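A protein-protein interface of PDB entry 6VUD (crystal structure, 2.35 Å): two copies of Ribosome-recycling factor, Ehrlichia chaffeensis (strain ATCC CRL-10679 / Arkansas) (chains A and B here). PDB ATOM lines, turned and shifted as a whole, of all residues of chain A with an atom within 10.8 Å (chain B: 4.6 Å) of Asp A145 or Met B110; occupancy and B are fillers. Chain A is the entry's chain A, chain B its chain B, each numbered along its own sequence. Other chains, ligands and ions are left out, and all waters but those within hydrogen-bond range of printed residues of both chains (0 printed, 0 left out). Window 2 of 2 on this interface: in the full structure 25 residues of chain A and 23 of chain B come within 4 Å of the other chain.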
ATOM      1  N   ILE A   3      18.357   4.226 -27.766  1.00  0.00           N
ATOM      2  CA  ILE A   3      18.229   4.820 -29.097  1.00  0.00           C
ATOM      3  C   ILE A   3      18.881   3.927 -30.147  1.00  0.00           C
ATOM      4  O   ILE A   3      18.426   3.870 -31.298  1.00  0.00           O
ATOM      5  CB  ILE A   3      18.825   6.247 -29.113  1.00  0.00           C
ATOM      6  CG1 ILE A   3      17.892   7.233 -28.412  1.00  0.00           C
ATOM      7  CG2 ILE A   3      19.084   6.730 -30.531  1.00  0.00           C
ATOM      8  CD1 ILE A   3      18.307   8.681 -28.574  1.00  0.00           C
ATOM      9  N   MET A 137       9.980   8.567 -35.111  1.00  0.00           N
ATOM     10  CA  MET A 137      10.061   9.802 -34.339  1.00  0.00           C
ATOM     11  C   MET A 137       9.065   9.796 -33.185  1.00  0.00           C
ATOM     12  O   MET A 137       9.393  10.223 -32.072  1.00  0.00           O
ATOM     13  CB  MET A 137       9.832  11.010 -35.248  1.00  0.00           C
ATOM     14  CG  MET A 137      10.807  11.117 -36.419  1.00  0.00           C
ATOM     15  SD  MET A 137      12.510  11.535 -35.961  1.00  0.00           S
ATOM     16  CE  MET A 137      13.243   9.923 -35.706  1.00  0.00           C
ATOM     17  N   ASP A 138       7.839   9.320 -33.431  1.00  0.00           N
ATOM     18  CA  ASP A 138       6.855   9.209 -32.358  1.00  0.00           C
ATOM     19  C   ASP A 138       7.391   8.371 -31.207  1.00  0.00           C
ATOM     20  O   ASP A 138       7.166   8.693 -30.037  1.00  0.00           O
ATOM     21  CB  ASP A 138       5.553   8.614 -32.897  1.00  0.00           C
ATOM     22  CG  ASP A 138       4.842   9.542 -33.859  1.00  0.00           C
ATOM     23  OD1 ASP A 138       5.243  10.717 -33.950  1.00  0.00           O
ATOM     24  OD2 ASP A 138       3.886   9.098 -34.526  1.00  0.00           O
ATOM     25  N   ARG A 139       8.117   7.296 -31.519  1.00  0.00           N
ATOM     26  CA  ARG A 139       8.698   6.465 -30.472  1.00  0.00           C
ATOM     27  C   ARG A 139       9.765   7.220 -29.690  1.00  0.00           C
ATOM     28  O   ARG A 139       9.880   7.055 -28.471  1.00  0.00           O
ATOM     29  CB  ARG A 139       9.286   5.191 -31.078  1.00  0.00           C
ATOM     30  CG  ARG A 139       8.255   4.287 -31.728  1.00  0.00           C
ATOM     31  CD  ARG A 139       8.914   3.030 -32.281  1.00  0.00           C
ATOM     32  NE  ARG A 139       9.588   2.275 -31.230  1.00  0.00           N
ATOM     33  CZ  ARG A 139      10.396   1.247 -31.451  1.00  0.00           C
ATOM     34  NH1 ARG A 139      10.639   0.850 -32.691  1.00  0.00           N
ATOM     35  NH2 ARG A 139      10.965   0.618 -30.429  1.00  0.00           N
ATOM     36  N   LEU A 140      10.560   8.044 -30.371  1.00  0.00           N
ATOM     37  CA  LEU A 140      11.585   8.806 -29.666  1.00  0.00           C
ATOM     38  C   LEU A 140      10.962   9.922 -28.841  1.00  0.00           C
ATOM     39  O   LEU A 140      11.447  10.237 -27.745  1.00  0.00           O
ATOM     40  CB  LEU A 140      12.611   9.364 -30.656  1.00  0.00           C
ATOM     41  CG  LEU A 140      13.594   8.372 -31.284  1.00  0.00           C
ATOM     42  CD1 LEU A 140      14.623   9.114 -32.115  1.00  0.00           C
ATOM     43  CD2 LEU A 140      14.278   7.537 -30.212  1.00  0.00           C
ATOM     44  N   LYS A 141       9.881  10.529 -29.344  1.00  0.00           N
ATOM     45  CA  LYS A 141       9.149  11.502 -28.538  1.00  0.00           C
ATOM     46  C   LYS A 141       8.594  10.854 -27.274  1.00  0.00           C
ATOM     47  O   LYS A 141       8.519  11.498 -26.222  1.00  0.00           O
ATOM     48  CB  LYS A 141       8.027  12.137 -29.357  1.00  0.00           C
ATOM     49  N   VAL A 142       8.212   9.572 -27.354  1.00  0.00           N
ATOM     50  CA  VAL A 142       7.779   8.854 -26.155  1.00  0.00           C
ATOM     51  C   VAL A 142       8.931   8.740 -25.166  1.00  0.00           C
ATOM     52  O   VAL A 142       8.786   9.063 -23.981  1.00  0.00           O
ATOM     53  CB  VAL A 142       7.212   7.468 -26.515  1.00  0.00           C
ATOM     54  CG1 VAL A 142       6.976   6.656 -25.241  1.00  0.00           C
ATOM     55  CG2 VAL A 142       5.921   7.603 -27.291  1.00  0.00           C
ATOM     56  N   MET A 143      10.097   8.284 -25.645  1.00  0.00           N
ATOM     57  CA  MET A 143      11.273   8.149 -24.789  1.00  0.00           C
ATOM     58  C   MET A 143      11.659   9.488 -24.174  1.00  0.00           C
ATOM     59  O   MET A 143      11.977   9.569 -22.981  1.00  0.00           O
ATOM     60  CB  MET A 143      12.451   7.566 -25.583  1.00  0.00           C
ATOM     61  CG  MET A 143      12.318   6.082 -25.920  1.00  0.00           C
ATOM     62  SD  MET A 143      13.459   5.465 -27.191  1.00  0.00           S
ATOM     63  CE  MET A 143      14.912   5.093 -26.205  1.00  0.00           C
ATOM     64  N   GLN A 144      11.628  10.555 -24.974  1.00  0.00           N
ATOM     65  CA  GLN A 144      12.028  11.863 -24.470  1.00  0.00           C
ATOM     66  C   GLN A 144      10.988  12.430 -23.508  1.00  0.00           C
ATOM     67  O   GLN A 144      11.341  13.118 -22.548  1.00  0.00           O
ATOM     68  CB  GLN A 144      12.286  12.815 -25.638  1.00  0.00           C
ATOM     69  CG  GLN A 144      12.713  14.221 -25.223  1.00  0.00           C
ATOM     70  CD  GLN A 144      11.598  15.235 -25.411  1.00  0.00           C
ATOM     71  OE1 GLN A 144      10.688  15.341 -24.580  1.00  0.00           O
ATOM     72  NE2 GLN A 144      11.656  15.981 -26.515  1.00  0.00           N
ATOM     73  N   ASP A 145       9.701  12.157 -23.747  1.00  0.00           N
ATOM     74  CA  ASP A 145       8.676  12.554 -22.785  1.00  0.00           C
ATOM     75  C   ASP A 145       8.766  11.715 -21.522  1.00  0.00           C
ATOM     76  O   ASP A 145       8.663  12.244 -20.408  1.00  0.00           O
ATOM     77  CB  ASP A 145       7.283  12.426 -23.395  1.00  0.00           C
ATOM     78  CG  ASP A 145       6.992  13.502 -24.410  1.00  0.00           C
ATOM     79  OD1 ASP A 145       7.929  14.261 -24.747  1.00  0.00           O
ATOM     80  OD2 ASP A 145       5.829  13.595 -24.864  1.00  0.00           O
ATOM     81  N   SER A 146       8.977  10.411 -21.672  1.00  0.00           N
ATOM     82  CA  SER A 146       9.190   9.528 -20.527  1.00  0.00           C
ATOM     83  C   SER A 146      10.506   9.840 -19.763  1.00  0.00           C
ATOM     84  O   SER A 146      10.832   9.080 -18.839  1.00  0.00           O
ATOM     85  CB  SER A 146       9.181   8.069 -20.991  1.00  0.00           C
ATOM     86  OG  SER A 146       7.982   7.747 -21.678  1.00  0.00           O
ATOM     87  N   LYS A 147      11.219  10.906 -20.148  1.00  0.00           N
ATOM     88  CA  LYS A 147      12.478  11.321 -19.522  1.00  0.00           C
ATOM     89  C   LYS A 147      13.566  10.260 -19.672  1.00  0.00           C
ATOM     90  O   LYS A 147      14.485  10.178 -18.852  1.00  0.00           O
ATOM     91  CB  LYS A 147      12.280  11.688 -18.046  1.00  0.00           C
ATOM     92  N   GLU A 148      13.476   9.445 -20.726  1.00  0.00           N
ATOM     93  CA  GLU A 148      14.488   8.432 -21.001  1.00  0.00           C
ATOM     94  C   GLU A 148      15.649   8.976 -21.814  1.00  0.00           C
ATOM     95  O   GLU A 148      16.778   8.493 -21.667  1.00  0.00           O
ATOM     96  CB  GLU A 148      13.873   7.248 -21.748  1.00  0.00           C
ATOM     97  CG  GLU A 148      12.670   6.642 -21.066  1.00  0.00           C
ATOM     98  CD  GLU A 148      12.223   5.368 -21.739  1.00  0.00           C
ATOM     99  OE1 GLU A 148      11.281   4.722 -21.233  1.00  0.00           O
ATOM    100  OE2 GLU A 148      12.821   5.013 -22.773  1.00  0.00           O
ATOM    101  N   ILE A 149      15.395   9.953 -22.685  1.00  0.00           N
ATOM    102  CA  ILE A 149      16.443  10.639 -23.423  1.00  0.00           C
ATOM    103  C   ILE A 149      16.178  12.137 -23.361  1.00  0.00           C
ATOM    104  O   ILE A 149      15.061  12.587 -23.096  1.00  0.00           O
ATOM    105  CB  ILE A 149      16.538  10.172 -24.889  1.00  0.00           C
ATOM    106  CG1 ILE A 149      15.256  10.529 -25.646  1.00  0.00           C
ATOM    107  CG2 ILE A 149      16.825   8.680 -24.947  1.00  0.00           C
ATOM    108  CD1 ILE A 149      15.316  10.231 -27.130  1.00  0.00           C
ATOM    109  N   SER A 150      17.233  12.909 -23.612  1.00  0.00           N
ATOM    110  CA  SER A 150      17.142  14.359 -23.595  1.00  0.00           C
ATOM    111  C   SER A 150      16.442  14.861 -24.856  1.00  0.00           C
ATOM    112  O   SER A 150      15.996  14.088 -25.710  1.00  0.00           O
ATOM    113  CB  SER A 150      18.533  14.975 -23.472  1.00  0.00           C
ATOM    114  OG  SER A 150      19.247  14.846 -24.691  1.00  0.00           O
ATOM    115  N   GLU A 151      16.333  16.184 -24.968  1.00  0.00           N
ATOM    116  CA  GLU A 151      15.888  16.779 -26.223  1.00  0.00           C
ATOM    117  C   GLU A 151      16.988  16.710 -27.274  1.00  0.00           C
ATOM    118  O   GLU A 151      16.710  16.492 -28.461  1.00  0.00           O
ATOM    119  CB  GLU A 151      15.456  18.225 -25.995  1.00  0.00           C
ATOM    120  CG  GLU A 151      15.111  18.974 -27.267  1.00  0.00           C
ATOM    121  CD  GLU A 151      13.806  18.512 -27.857  1.00  0.00           C
ATOM    122  OE1 GLU A 151      12.957  18.020 -27.086  1.00  0.00           O
ATOM    123  OE2 GLU A 151      13.630  18.633 -29.089  1.00  0.00           O
ATOM    124  N   ASP A 152      18.245  16.889 -26.854  1.00  0.00           N
ATOM    125  CA  ASP A 152      19.363  16.806 -27.790  1.00  0.00           C
ATOM    126  C   ASP A 152      19.430  15.434 -28.447  1.00  0.00           C
ATOM    127  O   ASP A 152      19.733  15.323 -29.640  1.00  0.00           O
ATOM    128  CB  ASP A 152      20.675  17.126 -27.069  1.00  0.00           C
ATOM    129  N   ASP A 153      19.132  14.374 -27.686  1.00  0.00           N
ATOM    130  CA  ASP A 153      19.122  13.033 -28.264  1.00  0.00           C
ATOM    131  C   ASP A 153      18.033  12.887 -29.317  1.00  0.00           C
ATOM    132  O   ASP A 153      18.162  12.064 -30.230  1.00  0.00           O
ATOM    133  CB  ASP A 153      18.931  11.977 -27.174  1.00  0.00           C
ATOM    134  CG  ASP A 153      20.000  12.036 -26.100  1.00  0.00           C
ATOM    135  OD1 ASP A 153      19.760  11.494 -24.999  1.00  0.00           O
ATOM    136  OD2 ASP A 153      21.069  12.633 -26.344  1.00  0.00           O
ATOM    137  N   LEU A 154      16.956  13.667 -29.209  1.00  0.00           N
ATOM    138  CA  LEU A 154      15.861  13.571 -30.168  1.00  0.00           C
ATOM    139  C   LEU A 154      16.203  14.285 -31.472  1.00  0.00           C
ATOM    140  O   LEU A 154      16.015  13.730 -32.561  1.00  0.00           O
ATOM    141  CB  LEU A 154      14.579  14.143 -29.557  1.00  0.00           C
ATOM    142  CG  LEU A 154      13.266  13.951 -30.321  1.00  0.00           C
ATOM    143  CD1 LEU A 154      12.112  13.895 -29.340  1.00  0.00           C
ATOM    144  CD2 LEU A 154      13.026  15.057 -31.342  1.00  0.00           C
ATOM    145  N   MET B 106       3.942   9.475 -12.759  1.00  0.00           N
ATOM    146  CA  MET B 106       3.683  10.142 -14.025  1.00  0.00           C
ATOM    147  C   MET B 106       2.850  11.383 -13.758  1.00  0.00           C
ATOM    148  O   MET B 106       1.786  11.296 -13.136  1.00  0.00           O
ATOM    149  CB  MET B 106       2.965   9.194 -14.982  1.00  0.00           C
ATOM    150  CG  MET B 106       2.605   9.787 -16.314  1.00  0.00           C
ATOM    151  SD  MET B 106       1.819   8.522 -17.316  1.00  0.00           S
ATOM    152  CE  MET B 106       0.534   7.960 -16.206  1.00  0.00           C
ATOM    153  N   THR B 107       3.338  12.532 -14.217  1.00  0.00           N
ATOM    154  CA  THR B 107       2.570  13.755 -14.070  1.00  0.00           C
ATOM    155  C   THR B 107       1.391  13.758 -15.039  1.00  0.00           C
ATOM    156  O   THR B 107       1.340  12.992 -16.009  1.00  0.00           O
ATOM    157  CB  THR B 107       3.449  14.980 -14.312  1.00  0.00           C
ATOM    158  OG1 THR B 107       3.809  15.048 -15.695  1.00  0.00           O
ATOM    159  CG2 THR B 107       4.709  14.898 -13.472  1.00  0.00           C
ATOM    160  N   GLN B 108       0.422  14.636 -14.756  1.00  0.00           N
ATOM    161  CA  GLN B 108      -0.721  14.776 -15.649  1.00  0.00           C
ATOM    162  C   GLN B 108      -0.300  15.338 -16.998  1.00  0.00           C
ATOM    163  O   GLN B 108      -0.953  15.066 -18.010  1.00  0.00           O
ATOM    164  CB  GLN B 108      -1.789  15.665 -15.011  1.00  0.00           C
ATOM    165  N   ASP B 109       0.792  16.106 -17.038  1.00  0.00           N
ATOM    166  CA  ASP B 109       1.270  16.623 -18.315  1.00  0.00           C
ATOM    167  C   ASP B 109       1.949  15.534 -19.135  1.00  0.00           C
ATOM    168  O   ASP B 109       1.735  15.450 -20.351  1.00  0.00           O
ATOM    169  CB  ASP B 109       2.206  17.805 -18.085  1.00  0.00           C
ATOM    170  CG  ASP B 109       1.453  19.120 -18.009  1.00  0.00           C
ATOM    171  OD1 ASP B 109       0.697  19.424 -18.961  1.00  0.00           O
ATOM    172  OD2 ASP B 109       1.595  19.834 -16.992  1.00  0.00           O
ATOM    173  N   MET B 110       2.768  14.693 -18.494  1.00  0.00           N
ATOM    174  CA  MET B 110       3.309  13.521 -19.176  1.00  0.00           C
ATOM    175  C   MET B 110       2.185  12.643 -19.707  1.00  0.00           C
ATOM    176  O   MET B 110       2.131  12.345 -20.903  1.00  0.00           O
ATOM    177  CB  MET B 110       4.201  12.714 -18.234  1.00  0.00           C
ATOM    178  CG  MET B 110       5.500  13.386 -17.848  1.00  0.00           C
ATOM    179  SD  MET B 110       6.475  12.334 -16.748  1.00  0.00           S
ATOM    180  CE  MET B 110       6.594  10.856 -17.766  1.00  0.00           C
ATOM    181  N   ARG B 111       1.263  12.242 -18.826  1.00  0.00           N
ATOM    182  CA  ARG B 111       0.120  11.425 -19.231  1.00  0.00           C
ATOM    183  C   ARG B 111      -0.637  12.041 -20.403  1.00  0.00           C
ATOM    184  O   ARG B 111      -1.017  11.330 -21.343  1.00  0.00           O
ATOM    185  CB  ARG B 111      -0.817  11.218 -18.040  1.00  0.00           C
ATOM    186  CG  ARG B 111      -2.126  10.518 -18.368  1.00  0.00           C
ATOM    187  CD  ARG B 111      -3.025  10.419 -17.124  1.00  0.00           C
ATOM    188  NE  ARG B 111      -2.439   9.597 -16.062  1.00  0.00           N
ATOM    189  CZ  ARG B 111      -1.951  10.075 -14.923  1.00  0.00           C
ATOM    190  NH1 ARG B 111      -1.984  11.378 -14.678  1.00  0.00           N
ATOM    191  NH2 ARG B 111      -1.438   9.245 -14.022  1.00  0.00           N
ATOM    192  N   LYS B 112      -0.869  13.358 -20.367  1.00  0.00           N
ATOM    193  CA  LYS B 112      -1.520  14.024 -21.495  1.00  0.00           C
ATOM    194  C   LYS B 112      -0.712  13.844 -22.778  1.00  0.00           C
ATOM    195  O   LYS B 112      -1.267  13.538 -23.836  1.00  0.00           O
ATOM    196  CB  LYS B 112      -1.720  15.509 -21.188  1.00  0.00           C
ATOM    197  N   ASN B 113       0.609  14.021 -22.695  1.00  0.00           N
ATOM    198  CA  ASN B 113       1.457  13.864 -23.873  1.00  0.00           C
ATOM    199  C   ASN B 113       1.427  12.434 -24.390  1.00  0.00           C
ATOM    200  O   ASN B 113       1.306  12.199 -25.600  1.00  0.00           O
ATOM    201  CB  ASN B 113       2.887  14.282 -23.548  1.00  0.00           C
ATOM    202  CG  ASN B 113       3.013  15.764 -23.322  1.00  0.00           C
ATOM    203  OD1 ASN B 113       2.325  16.555 -23.966  1.00  0.00           O
ATOM    204  ND2 ASN B 113       3.891  16.156 -22.403  1.00  0.00           N
ATOM    205  N   LEU B 114       1.537  11.460 -23.483  1.00  0.00           N
ATOM    206  CA  LEU B 114       1.549  10.065 -23.907  1.00  0.00           C
ATOM    207  C   LEU B 114       0.222   9.670 -24.549  1.00  0.00           C
ATOM    208  O   LEU B 114       0.202   8.929 -25.541  1.00  0.00           O
ATOM    209  CB  LEU B 114       1.895   9.170 -22.718  1.00  0.00           C
ATOM    210  CG  LEU B 114       3.360   9.330 -22.293  1.00  0.00           C
ATOM    211  CD1 LEU B 114       3.692   8.508 -21.060  1.00  0.00           C
ATOM    212  CD2 LEU B 114       4.282   8.950 -23.434  1.00  0.00           C
ATOM    213  N   LEU B 117       0.474  10.969 -28.034  1.00  0.00           N
ATOM    214  CA  LEU B 117       1.402  10.174 -28.836  1.00  0.00           C
ATOM    215  C   LEU B 117       0.843   8.786 -29.127  1.00  0.00           C
ATOM    216  O   LEU B 117       1.064   8.239 -30.217  1.00  0.00           O
ATOM    217  CB  LEU B 117       2.748  10.074 -28.129  1.00  0.00           C
ATOM    218  CG  LEU B 117       3.768  11.105 -28.601  1.00  0.00           C
ATOM    219  CD1 LEU B 117       4.968  11.171 -27.653  1.00  0.00           C
ATOM    220  CD2 LEU B 117       4.190  10.771 -30.029  1.00  0.00           C
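O of Val A142 lies within hydrogen-bond range of OG of Ser A146 (2.8 Å). The side-chain amide nitrogen (ND2) of Asn B113 sits at hydrogen-bond distance from the backbone carbonyl oxygen (O) of Asp B109. The side-chain amide oxygen (OE1) of Gln A144 lies close to the side-chain carboxylate (OD1) of Asp A145 (3.0 Å). The side-chain hydroxyl (OG1) of Thr B107 sits at hydrogen-bond distance from the backbone NH (N) of Met B110 (3.0 Å).
Among the printed residues, merely in contact across the chains: Asp A145 with Asn B113 (3.3 Å), Val A142 with Leu B117 (3.6 Å), Asp A138 with Leu B117 (3.6 Å), Asp A145 with Met B110 (3.6 Å), Lys A141 with Leu B117 (3.6 Å), Asp A145 with Leu B117 (3.8 Å) and Val A142 with Leu B114 (3.97 Å).
Of chain B, only Met B110, Asn B113 and Leu B117 come within 4 Å of Asp A145. Of the printed residues of chain A, Met B110 touches Asp A145 (3.6 Å). No residue of chain A comes within 4 Å of Met B106. Thr B107 touches none of the printed residues of chain A. No residue of chain A comes within 4 Å of Asp B109. Lys B112 touches none of the printed residues of chain A. Printed residues of chain A within 4 Å of Asn B113: Asp A145 (3.3 Å). Printed residues of chain B within 4 Å of Lys A141: Leu B117. Of the printed residues of chain B, Val A142 touches Leu B114 (3.97 Å) and Leu B117 (3.6 Å). The nearest printed residue of chain A that does not touch Met B110 is Ser A146 (4.02 Å). The nearest printed residue of chain B that does not touch Asp A138 is Leu B114 (7.2 Å).
Hydrophobic or aromatic side chains of chain B within 4 Å of the printed part of chain A: Met B110, Leu B114 and Leu B117. Hydrophobic or aromatic side chains of chain A within 4 Å of the printed part of chain B: Val A142. Among the printed residues, no Asp or Glu carboxylate lies within 4 Å of a Lys or Arg side-chain nitrogen of the other chain.
No position is printed for both chains.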
